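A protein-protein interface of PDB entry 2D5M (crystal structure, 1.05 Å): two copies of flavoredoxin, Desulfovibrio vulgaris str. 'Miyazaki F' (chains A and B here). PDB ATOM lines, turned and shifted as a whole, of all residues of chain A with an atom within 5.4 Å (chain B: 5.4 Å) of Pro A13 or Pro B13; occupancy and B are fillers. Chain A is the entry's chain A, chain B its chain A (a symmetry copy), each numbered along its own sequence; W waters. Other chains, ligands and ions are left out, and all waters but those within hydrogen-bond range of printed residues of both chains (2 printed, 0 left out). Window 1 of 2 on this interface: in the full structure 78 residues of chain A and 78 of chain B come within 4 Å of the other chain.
Of the 11 printed residues of chain B, 8 touch a printed residue of chain A. Hydrophobic or aromatic side chains of chain B that line the printed part of chain A: Tyr B12, Pro B13, Pro B15, Phe B17, Pro B161 and Ile B163. Along chain B the printed residues that touch a printed residue of chain A span positions 12 to 163. Of the 11 printed residues of chain A, 8 touch a printed residue of chain B. Printed residues of chain A that touch a printed residue of chain B: Tyr A12, Pro A13, Thr A14, Pro A15, Phe A17, Pro A161, Val A162 and Ile A163. Among the printed residues, 12 pairs touch across the chains. Among the printed residues, no Asp or Glu carboxylate lies within 4 Å of a Lys or Arg side-chain nitrogen of the other chain.
Water W2 bridges the backbone carbonyl oxygen of Tyr B12 (2.7 Å) and the backbone NH of Leu A16 (3.0 Å). Water W1 lies within hydrogen-bond range of O of Tyr A12 (2.7 Å) and N of Leu B16 (3.0 Å).
Tyr A12 touches Phe B17, and with the chains exchanged Phe A17 touches Tyr B12. Tyr A12 touches Pro B161, and with the chains exchanged Pro A161 touches Tyr B12. Pro A13 touches Thr B14, and with the chains exchanged Thr A14 touches Pro B13. Pro A13 touches Pro B15, and with the chains exchanged Pro A15 touches Pro B13. 11 positions are printed for both chains. Of the 12 pairs that touch across the chains among the printed residues, 12 have their exchanged pair printed and touching as well.
The backbone carbonyl oxygen (O) of Phe A164 sits at hydrogen-bond distance from the side-chain hydroxyl (OG1) of Thr A14 (2.8 Å). The side-chain hydroxyl of Thr B14 is in hydrogen-bond range of the backbone carbonyl oxygen of Phe B164, 2.8 Å away.
Phe B17 touches Tyr A12 (CE2 to O, 3.7 Å). CG of Pro B161 touches CB of Tyr A12 (3.8 Å). Pro B13 touches Pro A13. O of Thr B14 touches CG of Pro A13, at 3.7 Å. Pro B13 touches Thr A14 (CG to O, 3.7 Å). Pro B13 touches Pro A15 (CD to CA, 3.7 Å). CE2 of Phe A17 touches O of Tyr B12, 3.7 Å away. Pro A161 touches Tyr B12. CD of Pro B13 touches O of Val A162, at 3.8 Å. CD1 of Ile A163 touches CD1 of Ile B163, 3.5 Å away.
Of chain B, only Pro B13 (3.9 Å), Thr B14 (3.7 Å), Pro B15 (3.7 Å) and Val B162 (3.8 Å) come within 4 Å of Pro A13. Of the printed residues of chain B, Pro A15 touches Pro B13 (3.7 Å). Of the printed residues of chain B, Pro A161 touches Tyr B12. Printed residues of chain B within 4 Å of Ile A163: Ile B163. Pro B13 touches just these residues of chain A: Pro A13, Thr A14, Pro A15 and Val A162. Of the printed residues of chain A, Pro B15 touches Pro A13 (3.7 Å). Of the printed residues of chain A, Ile B163 touches Ile A163 (3.5 Å). The nearest residue of chain B that does not touch Pro A13 is Ile B163 (4.1 Å). The nearest residue of chain A that does not touch Pro B13 is Ile A163 (4.1 Å).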
ATOM      1  N   ALA A  11      13.322 -14.243  26.300  1.00  0.00           N
ATOM      2  CA  ALA A  11      12.037 -14.885  26.404  1.00  0.00           C
ATOM      3  C   ALA A  11      12.205 -16.346  26.020  1.00  0.00           C
ATOM      4  O   ALA A  11      13.170 -16.669  25.311  1.00  0.00           O
ATOM      5  CB  ALA A  11      10.992 -14.226  25.532  1.00  0.00           C
ATOM      6  N   TYR A  12      11.293 -17.209  26.471  1.00  0.00           N
ATOM      7  CA  TYR A  12      11.369 -18.622  26.142  1.00  0.00           C
ATOM      8  C   TYR A  12       9.955 -19.137  25.869  1.00  0.00           C
ATOM      9  O   TYR A  12       9.013 -18.658  26.538  1.00  0.00           O
ATOM     10  CB  TYR A  12      11.856 -19.475  27.283  1.00  0.00           C
ATOM     11  CG  TYR A  12      13.140 -19.061  27.928  1.00  0.00           C
ATOM     12  CD1 TYR A  12      14.341 -18.989  27.190  1.00  0.00           C
ATOM     13  CD2 TYR A  12      13.192 -18.731  29.251  1.00  0.00           C
ATOM     14  CE1 TYR A  12      15.510 -18.604  27.776  1.00  0.00           C
ATOM     15  CE2 TYR A  12      14.388 -18.383  29.852  1.00  0.00           C
ATOM     16  CZ  TYR A  12      15.537 -18.315  29.136  1.00  0.00           C
ATOM     17  OH  TYR A  12      16.715 -17.936  29.748  1.00  0.00           O
ATOM     18  N   PRO A  13       9.789 -20.125  25.007  1.00  0.00           N
ATOM     19  CA  PRO A  13      10.775 -20.583  24.021  1.00  0.00           C
ATOM     20  C   PRO A  13      10.903 -19.545  22.920  1.00  0.00           C
ATOM     21  O   PRO A  13      10.029 -18.719  22.730  1.00  0.00           O
ATOM     22  CB  PRO A  13      10.128 -21.851  23.454  1.00  0.00           C
ATOM     23  CG  PRO A  13       8.674 -21.497  23.486  1.00  0.00           C
ATOM     24  CD  PRO A  13       8.488 -20.797  24.808  1.00  0.00           C
ATOM     25  N   THR A  14      11.998 -19.656  22.158  1.00  0.00           N
ATOM     26  CA  THR A  14      12.106 -19.024  20.829  1.00  0.00           C
ATOM     27  C   THR A  14      12.410 -20.133  19.837  1.00  0.00           C
ATOM     28  O   THR A  14      13.020 -21.157  20.216  1.00  0.00           O
ATOM     29  CB  THR A  14      13.117 -17.853  20.737  1.00  0.00           C
ATOM     30  OG1 THR A  14      14.453 -18.344  20.678  1.00  0.00           O
ATOM     31  CG2 THR A  14      12.941 -16.909  21.924  1.00  0.00           C
ATOM     32  N   PRO A  15      11.983 -19.983  18.597  1.00  0.00           N
ATOM     33  CA  PRO A  15      12.191 -21.044  17.606  1.00  0.00           C
ATOM     34  C   PRO A  15      13.562 -20.966  16.991  1.00  0.00           C
ATOM     35  O   PRO A  15      14.348 -20.017  17.140  1.00  0.00           O
ATOM     36  CB  PRO A  15      11.093 -20.747  16.596  1.00  0.00           C
ATOM     37  CG  PRO A  15      10.988 -19.263  16.611  1.00  0.00           C
ATOM     38  CD  PRO A  15      11.191 -18.864  18.039  1.00  0.00           C
ATOM     39  N   LEU A  16      13.860 -22.012  16.216  1.00  0.00           N
ATOM     40  CA  LEU A  16      15.049 -22.056  15.383  1.00  0.00           C
ATOM     41  C   LEU A  16      14.588 -22.460  13.994  1.00  0.00           C
ATOM     42  O   LEU A  16      14.602 -23.634  13.610  1.00  0.00           O
ATOM     43  CB  LEU A  16      16.134 -23.030  15.937  1.00  0.00           C
ATOM     44  CG  LEU A  16      17.454 -23.066  15.146  1.00  0.00           C
ATOM     45  CD1 LEU A  16      18.126 -21.719  15.184  1.00  0.00           C
ATOM     46  CD2 LEU A  16      18.361 -24.173  15.669  1.00  0.00           C
ATOM     47  N   PHE A  17      14.105 -21.481  13.241  1.00  0.00           N
ATOM     48  CA  PHE A  17      13.632 -21.693  11.889  1.00  0.00           C
ATOM     49  C   PHE A  17      14.777 -21.553  10.888  1.00  0.00           C
ATOM     50  O   PHE A  17      15.488 -20.576  10.916  1.00  0.00           O
ATOM     51  CB  PHE A  17      12.581 -20.641  11.560  1.00  0.00           C
ATOM     52  CG  PHE A  17      11.265 -20.772  12.353  1.00  0.00           C
ATOM     53  CD1 PHE A  17      10.434 -19.655  12.440  1.00  0.00           C
ATOM     54  CD2 PHE A  17      10.840 -21.945  12.981  1.00  0.00           C
ATOM     55  CE1 PHE A  17       9.211 -19.666  13.065  1.00  0.00           C
ATOM     56  CE2 PHE A  17       9.571 -21.951  13.611  1.00  0.00           C
ATOM     57  CZ  PHE A  17       8.753 -20.842  13.648  1.00  0.00           C
ATOM     58  N   PRO A 161      11.865 -30.832  17.452  1.00  0.00           N
ATOM     59  CA  PRO A 161      12.393 -29.524  17.031  1.00  0.00           C
ATOM     60  C   PRO A 161      13.328 -28.889  18.061  1.00  0.00           C
ATOM     61  O   PRO A 161      13.288 -29.182  19.254  1.00  0.00           O
ATOM     62  CB  PRO A 161      11.110 -28.680  16.933  1.00  0.00           C
ATOM     63  CG  PRO A 161      10.213 -29.241  17.994  1.00  0.00           C
ATOM     64  CD  PRO A 161      10.471 -30.724  17.951  1.00  0.00           C
ATOM     65  N   VAL A 162      14.185 -28.009  17.579  1.00  0.00           N
ATOM     66  CA  VAL A 162      15.122 -27.304  18.438  1.00  0.00           C
ATOM     67  C   VAL A 162      14.508 -26.011  18.940  1.00  0.00           C
ATOM     68  O   VAL A 162      13.859 -25.262  18.202  1.00  0.00           O
ATOM     69  CB  VAL A 162      16.425 -27.023  17.690  1.00  0.00           C
ATOM     70  CG1 VAL A 162      17.439 -26.237  18.480  1.00  0.00           C
ATOM     71  CG2 VAL A 162      17.098 -28.281  17.167  1.00  0.00           C
ATOM     72  N   ILE A 163      14.775 -25.703  20.187  1.00  0.00           N
ATOM     73  CA  ILE A 163      14.443 -24.492  20.860  1.00  0.00           C
ATOM     74  C   ILE A 163      15.689 -23.632  21.057  1.00  0.00           C
ATOM     75  O   ILE A 163      16.714 -24.161  21.483  1.00  0.00           O
ATOM     76  CB  ILE A 163      13.801 -24.717  22.285  1.00  0.00           C
ATOM     77  CG1 ILE A 163      12.513 -25.549  22.141  1.00  0.00           C
ATOM     78  CG2 ILE A 163      13.548 -23.513  23.080  1.00  0.00           C
ATOM     79  CD1 ILE A 163      12.223 -26.195  23.480  1.00  0.00           C
ATOM     80  N   PHE A 164      15.628 -22.323  20.814  1.00  0.00           N
ATOM     81  CA  PHE A 164      16.709 -21.416  21.078  1.00  0.00           C
ATOM     82  C   PHE A 164      16.477 -20.634  22.371  1.00  0.00           C
ATOM     83  O   PHE A 164      15.383 -20.115  22.596  1.00  0.00           O
ATOM     84  CB  PHE A 164      16.931 -20.467  19.909  1.00  0.00           C
ATOM     85  CG  PHE A 164      17.959 -19.377  20.082  1.00  0.00           C
ATOM     86  CD1 PHE A 164      19.301 -19.725  20.356  1.00  0.00           C
ATOM     87  CD2 PHE A 164      17.656 -18.062  19.991  1.00  0.00           C
ATOM     88  CE1 PHE A 164      20.261 -18.765  20.469  1.00  0.00           C
ATOM     89  CE2 PHE A 164      18.609 -17.087  20.049  1.00  0.00           C
ATOM     90  CZ  PHE A 164      19.934 -17.424  20.316  1.00  0.00           C
ATOM     91  N   ALA B  11       3.645 -24.815  13.501  1.00  0.00           N
ATOM     92  CA  ALA B  11       5.061 -24.603  13.654  1.00  0.00           C
ATOM     93  C   ALA B  11       5.436 -24.916  15.093  1.00  0.00           C
ATOM     94  O   ALA B  11       4.555 -24.866  15.963  1.00  0.00           O
ATOM     95  CB  ALA B  11       5.473 -23.193  13.295  1.00  0.00           C
ATOM     96  N   TYR B  12       6.709 -25.231  15.342  1.00  0.00           N
ATOM     97  CA  TYR B  12       7.158 -25.532  16.691  1.00  0.00           C
ATOM     98  C   TYR B  12       8.538 -24.906  16.897  1.00  0.00           C
ATOM     99  O   TYR B  12       9.324 -24.875  15.924  1.00  0.00           O
ATOM    100  CB  TYR B  12       7.382 -27.002  16.930  1.00  0.00           C
ATOM    101  CG  TYR B  12       6.251 -27.917  16.583  1.00  0.00           C
ATOM    102  CD1 TYR B  12       4.989 -27.791  17.203  1.00  0.00           C
ATOM    103  CD2 TYR B  12       6.399 -28.899  15.648  1.00  0.00           C
ATOM    104  CE1 TYR B  12       3.957 -28.620  16.881  1.00  0.00           C
ATOM    105  CE2 TYR B  12       5.362 -29.767  15.356  1.00  0.00           C
ATOM    106  CZ  TYR B  12       4.153 -29.639  15.955  1.00  0.00           C
ATOM    107  OH  TYR B  12       3.120 -30.495  15.627  1.00  0.00           O
ATOM    108  N   PRO B  13       8.883 -24.505  18.108  1.00  0.00           N
ATOM    109  CA  PRO B  13       7.971 -24.287  19.236  1.00  0.00           C
ATOM    110  C   PRO B  13       7.143 -23.039  18.980  1.00  0.00           C
ATOM    111  O   PRO B  13       7.507 -22.198  18.178  1.00  0.00           O
ATOM    112  CB  PRO B  13       8.927 -24.032  20.405  1.00  0.00           C
ATOM    113  CG  PRO B  13      10.052 -23.307  19.733  1.00  0.00           C
ATOM    114  CD  PRO B  13      10.250 -24.048  18.435  1.00  0.00           C
ATOM    115  N   THR B  14       6.046 -22.919  19.735  1.00  0.00           N
ATOM    116  CA  THR B  14       5.350 -21.631  19.922  1.00  0.00           C
ATOM    117  C   THR B  14       5.305 -21.368  21.418  1.00  0.00           C
ATOM    118  O   THR B  14       5.302 -22.329  22.219  1.00  0.00           O
ATOM    119  CB  THR B  14       3.951 -21.536  19.262  1.00  0.00           C
ATOM    120  OG1 THR B  14       2.982 -22.241  20.032  1.00  0.00           O
ATOM    121  CG2 THR B  14       4.003 -22.077  17.835  1.00  0.00           C
ATOM    122  N   PRO B  15       5.301 -20.112  21.821  1.00  0.00           N
ATOM    123  CA  PRO B  15       5.319 -19.790  23.252  1.00  0.00           C
ATOM    124  C   PRO B  15       3.938 -19.835  23.848  1.00  0.00           C
ATOM    125  O   PRO B  15       2.890 -19.928  23.189  1.00  0.00           O
ATOM    126  CB  PRO B  15       5.895 -18.383  23.248  1.00  0.00           C
ATOM    127  CG  PRO B  15       5.363 -17.784  21.994  1.00  0.00           C
ATOM    128  CD  PRO B  15       5.376 -18.891  20.988  1.00  0.00           C
ATOM    129  N   LEU B  16       3.927 -19.724  25.178  1.00  0.00           N
ATOM    130  CA  LEU B  16       2.700 -19.559  25.939  1.00  0.00           C
ATOM    131  C   LEU B  16       2.923 -18.377  26.865  1.00  0.00           C
ATOM    132  O   LEU B  16       3.312 -18.515  28.030  1.00  0.00           O
ATOM    133  CB  LEU B  16       2.307 -20.846  26.730  1.00  0.00           C
ATOM    134  CG  LEU B  16       0.975 -20.768  27.496  1.00  0.00           C
ATOM    135  CD1 LEU B  16      -0.171 -20.569  26.539  1.00  0.00           C
ATOM    136  CD2 LEU B  16       0.785 -22.004  28.365  1.00  0.00           C
ATOM    137  N   PHE B  17       2.740 -17.180  26.325  1.00  0.00           N
ATOM    138  CA  PHE B  17       2.901 -15.950  27.072  1.00  0.00           C
ATOM    139  C   PHE B  17       1.594 -15.559  27.755  1.00  0.00           C
ATOM    140  O   PHE B  17       0.569 -15.509  27.118  1.00  0.00           O
ATOM    141  CB  PHE B  17       3.289 -14.833  26.110  1.00  0.00           C
ATOM    142  CG  PHE B  17       4.690 -14.978  25.482  1.00  0.00           C
ATOM    143  CD1 PHE B  17       4.961 -14.272  24.309  1.00  0.00           C
ATOM    144  CD2 PHE B  17       5.713 -15.762  26.017  1.00  0.00           C
ATOM    145  CE1 PHE B  17       6.188 -14.271  23.692  1.00  0.00           C
ATOM    146  CE2 PHE B  17       6.978 -15.746  25.381  1.00  0.00           C
ATOM    147  CZ  PHE B  17       7.231 -15.006  24.245  1.00  0.00           C
ATOM    148  N   PRO B 161       9.705 -23.263  31.291  1.00  0.00           N
ATOM    149  CA  PRO B 161       8.587 -22.642  30.565  1.00  0.00           C
ATOM    150  C   PRO B 161       7.763 -23.642  29.752  1.00  0.00           C
ATOM    151  O   PRO B 161       8.222 -24.716  29.373  1.00  0.00           O
ATOM    152  CB  PRO B 161       9.322 -21.695  29.598  1.00  0.00           C
ATOM    153  CG  PRO B 161      10.606 -22.402  29.291  1.00  0.00           C
ATOM    154  CD  PRO B 161      10.998 -23.043  30.598  1.00  0.00           C
ATOM    155  N   VAL B 162       6.524 -23.272  29.490  1.00  0.00           N
ATOM    156  CA  VAL B 162       5.625 -24.104  28.708  1.00  0.00           C
ATOM    157  C   VAL B 162       5.739 -23.763  27.234  1.00  0.00           C
ATOM    158  O   VAL B 162       5.802 -22.597  26.833  1.00  0.00           O
ATOM    159  CB  VAL B 162       4.184 -23.934  29.187  1.00  0.00           C
ATOM    160  CG1 VAL B 162       3.168 -24.712  28.393  1.00  0.00           C
ATOM    161  CG2 VAL B 162       3.999 -24.269  30.658  1.00  0.00           C
ATOM    162  N   ILE B 163       5.690 -24.783  26.411  1.00  0.00           N
ATOM    163  CA  ILE B 163       5.636 -24.733  24.988  1.00  0.00           C
ATOM    164  C   ILE B 163       4.237 -25.095  24.494  1.00  0.00           C
ATOM    165  O   ILE B 163       3.676 -26.080  24.969  1.00  0.00           O
ATOM    166  CB  ILE B 163       6.649 -25.719  24.283  1.00  0.00           C
ATOM    167  CG1 ILE B 163       8.086 -25.373  24.716  1.00  0.00           C
ATOM    168  CG2 ILE B 163       6.559 -25.805  22.823  1.00  0.00           C
ATOM    169  CD1 ILE B 163       8.948 -26.598  24.489  1.00  0.00           C
ATOM    170  N   PHE B 164       3.676 -24.369  23.527  1.00  0.00           N
ATOM    171  CA  PHE B 164       2.417 -24.696  22.918  1.00  0.00           C
ATOM    172  C   PHE B 164       2.614 -25.362  21.557  1.00  0.00           C
ATOM    173  O   PHE B 164       3.403 -24.887  20.740  1.00  0.00           O
ATOM    174  CB  PHE B 164       1.529 -23.468  22.793  1.00  0.00           C
ATOM    175  CG  PHE B 164       0.216 -23.629  22.067  1.00  0.00           C
ATOM    176  CD1 PHE B 164      -0.736 -24.554  22.551  1.00  0.00           C
ATOM    177  CD2 PHE B 164      -0.099 -22.924  20.956  1.00  0.00           C
ATOM    178  CE1 PHE B 164      -1.950 -24.687  21.946  1.00  0.00           C
ATOM    179  CE2 PHE B 164      -1.327 -23.002  20.365  1.00  0.00           C
ATOM    180  CZ  PHE B 164      -2.270 -23.910  20.840  1.00  0.00           C
HETATM  181  O   HOH W   1       6.340 -18.960  26.812  1.00  0.00           O
HETATM  182  O   HOH W   2      11.847 -24.084  15.360  1.00  0.00           O
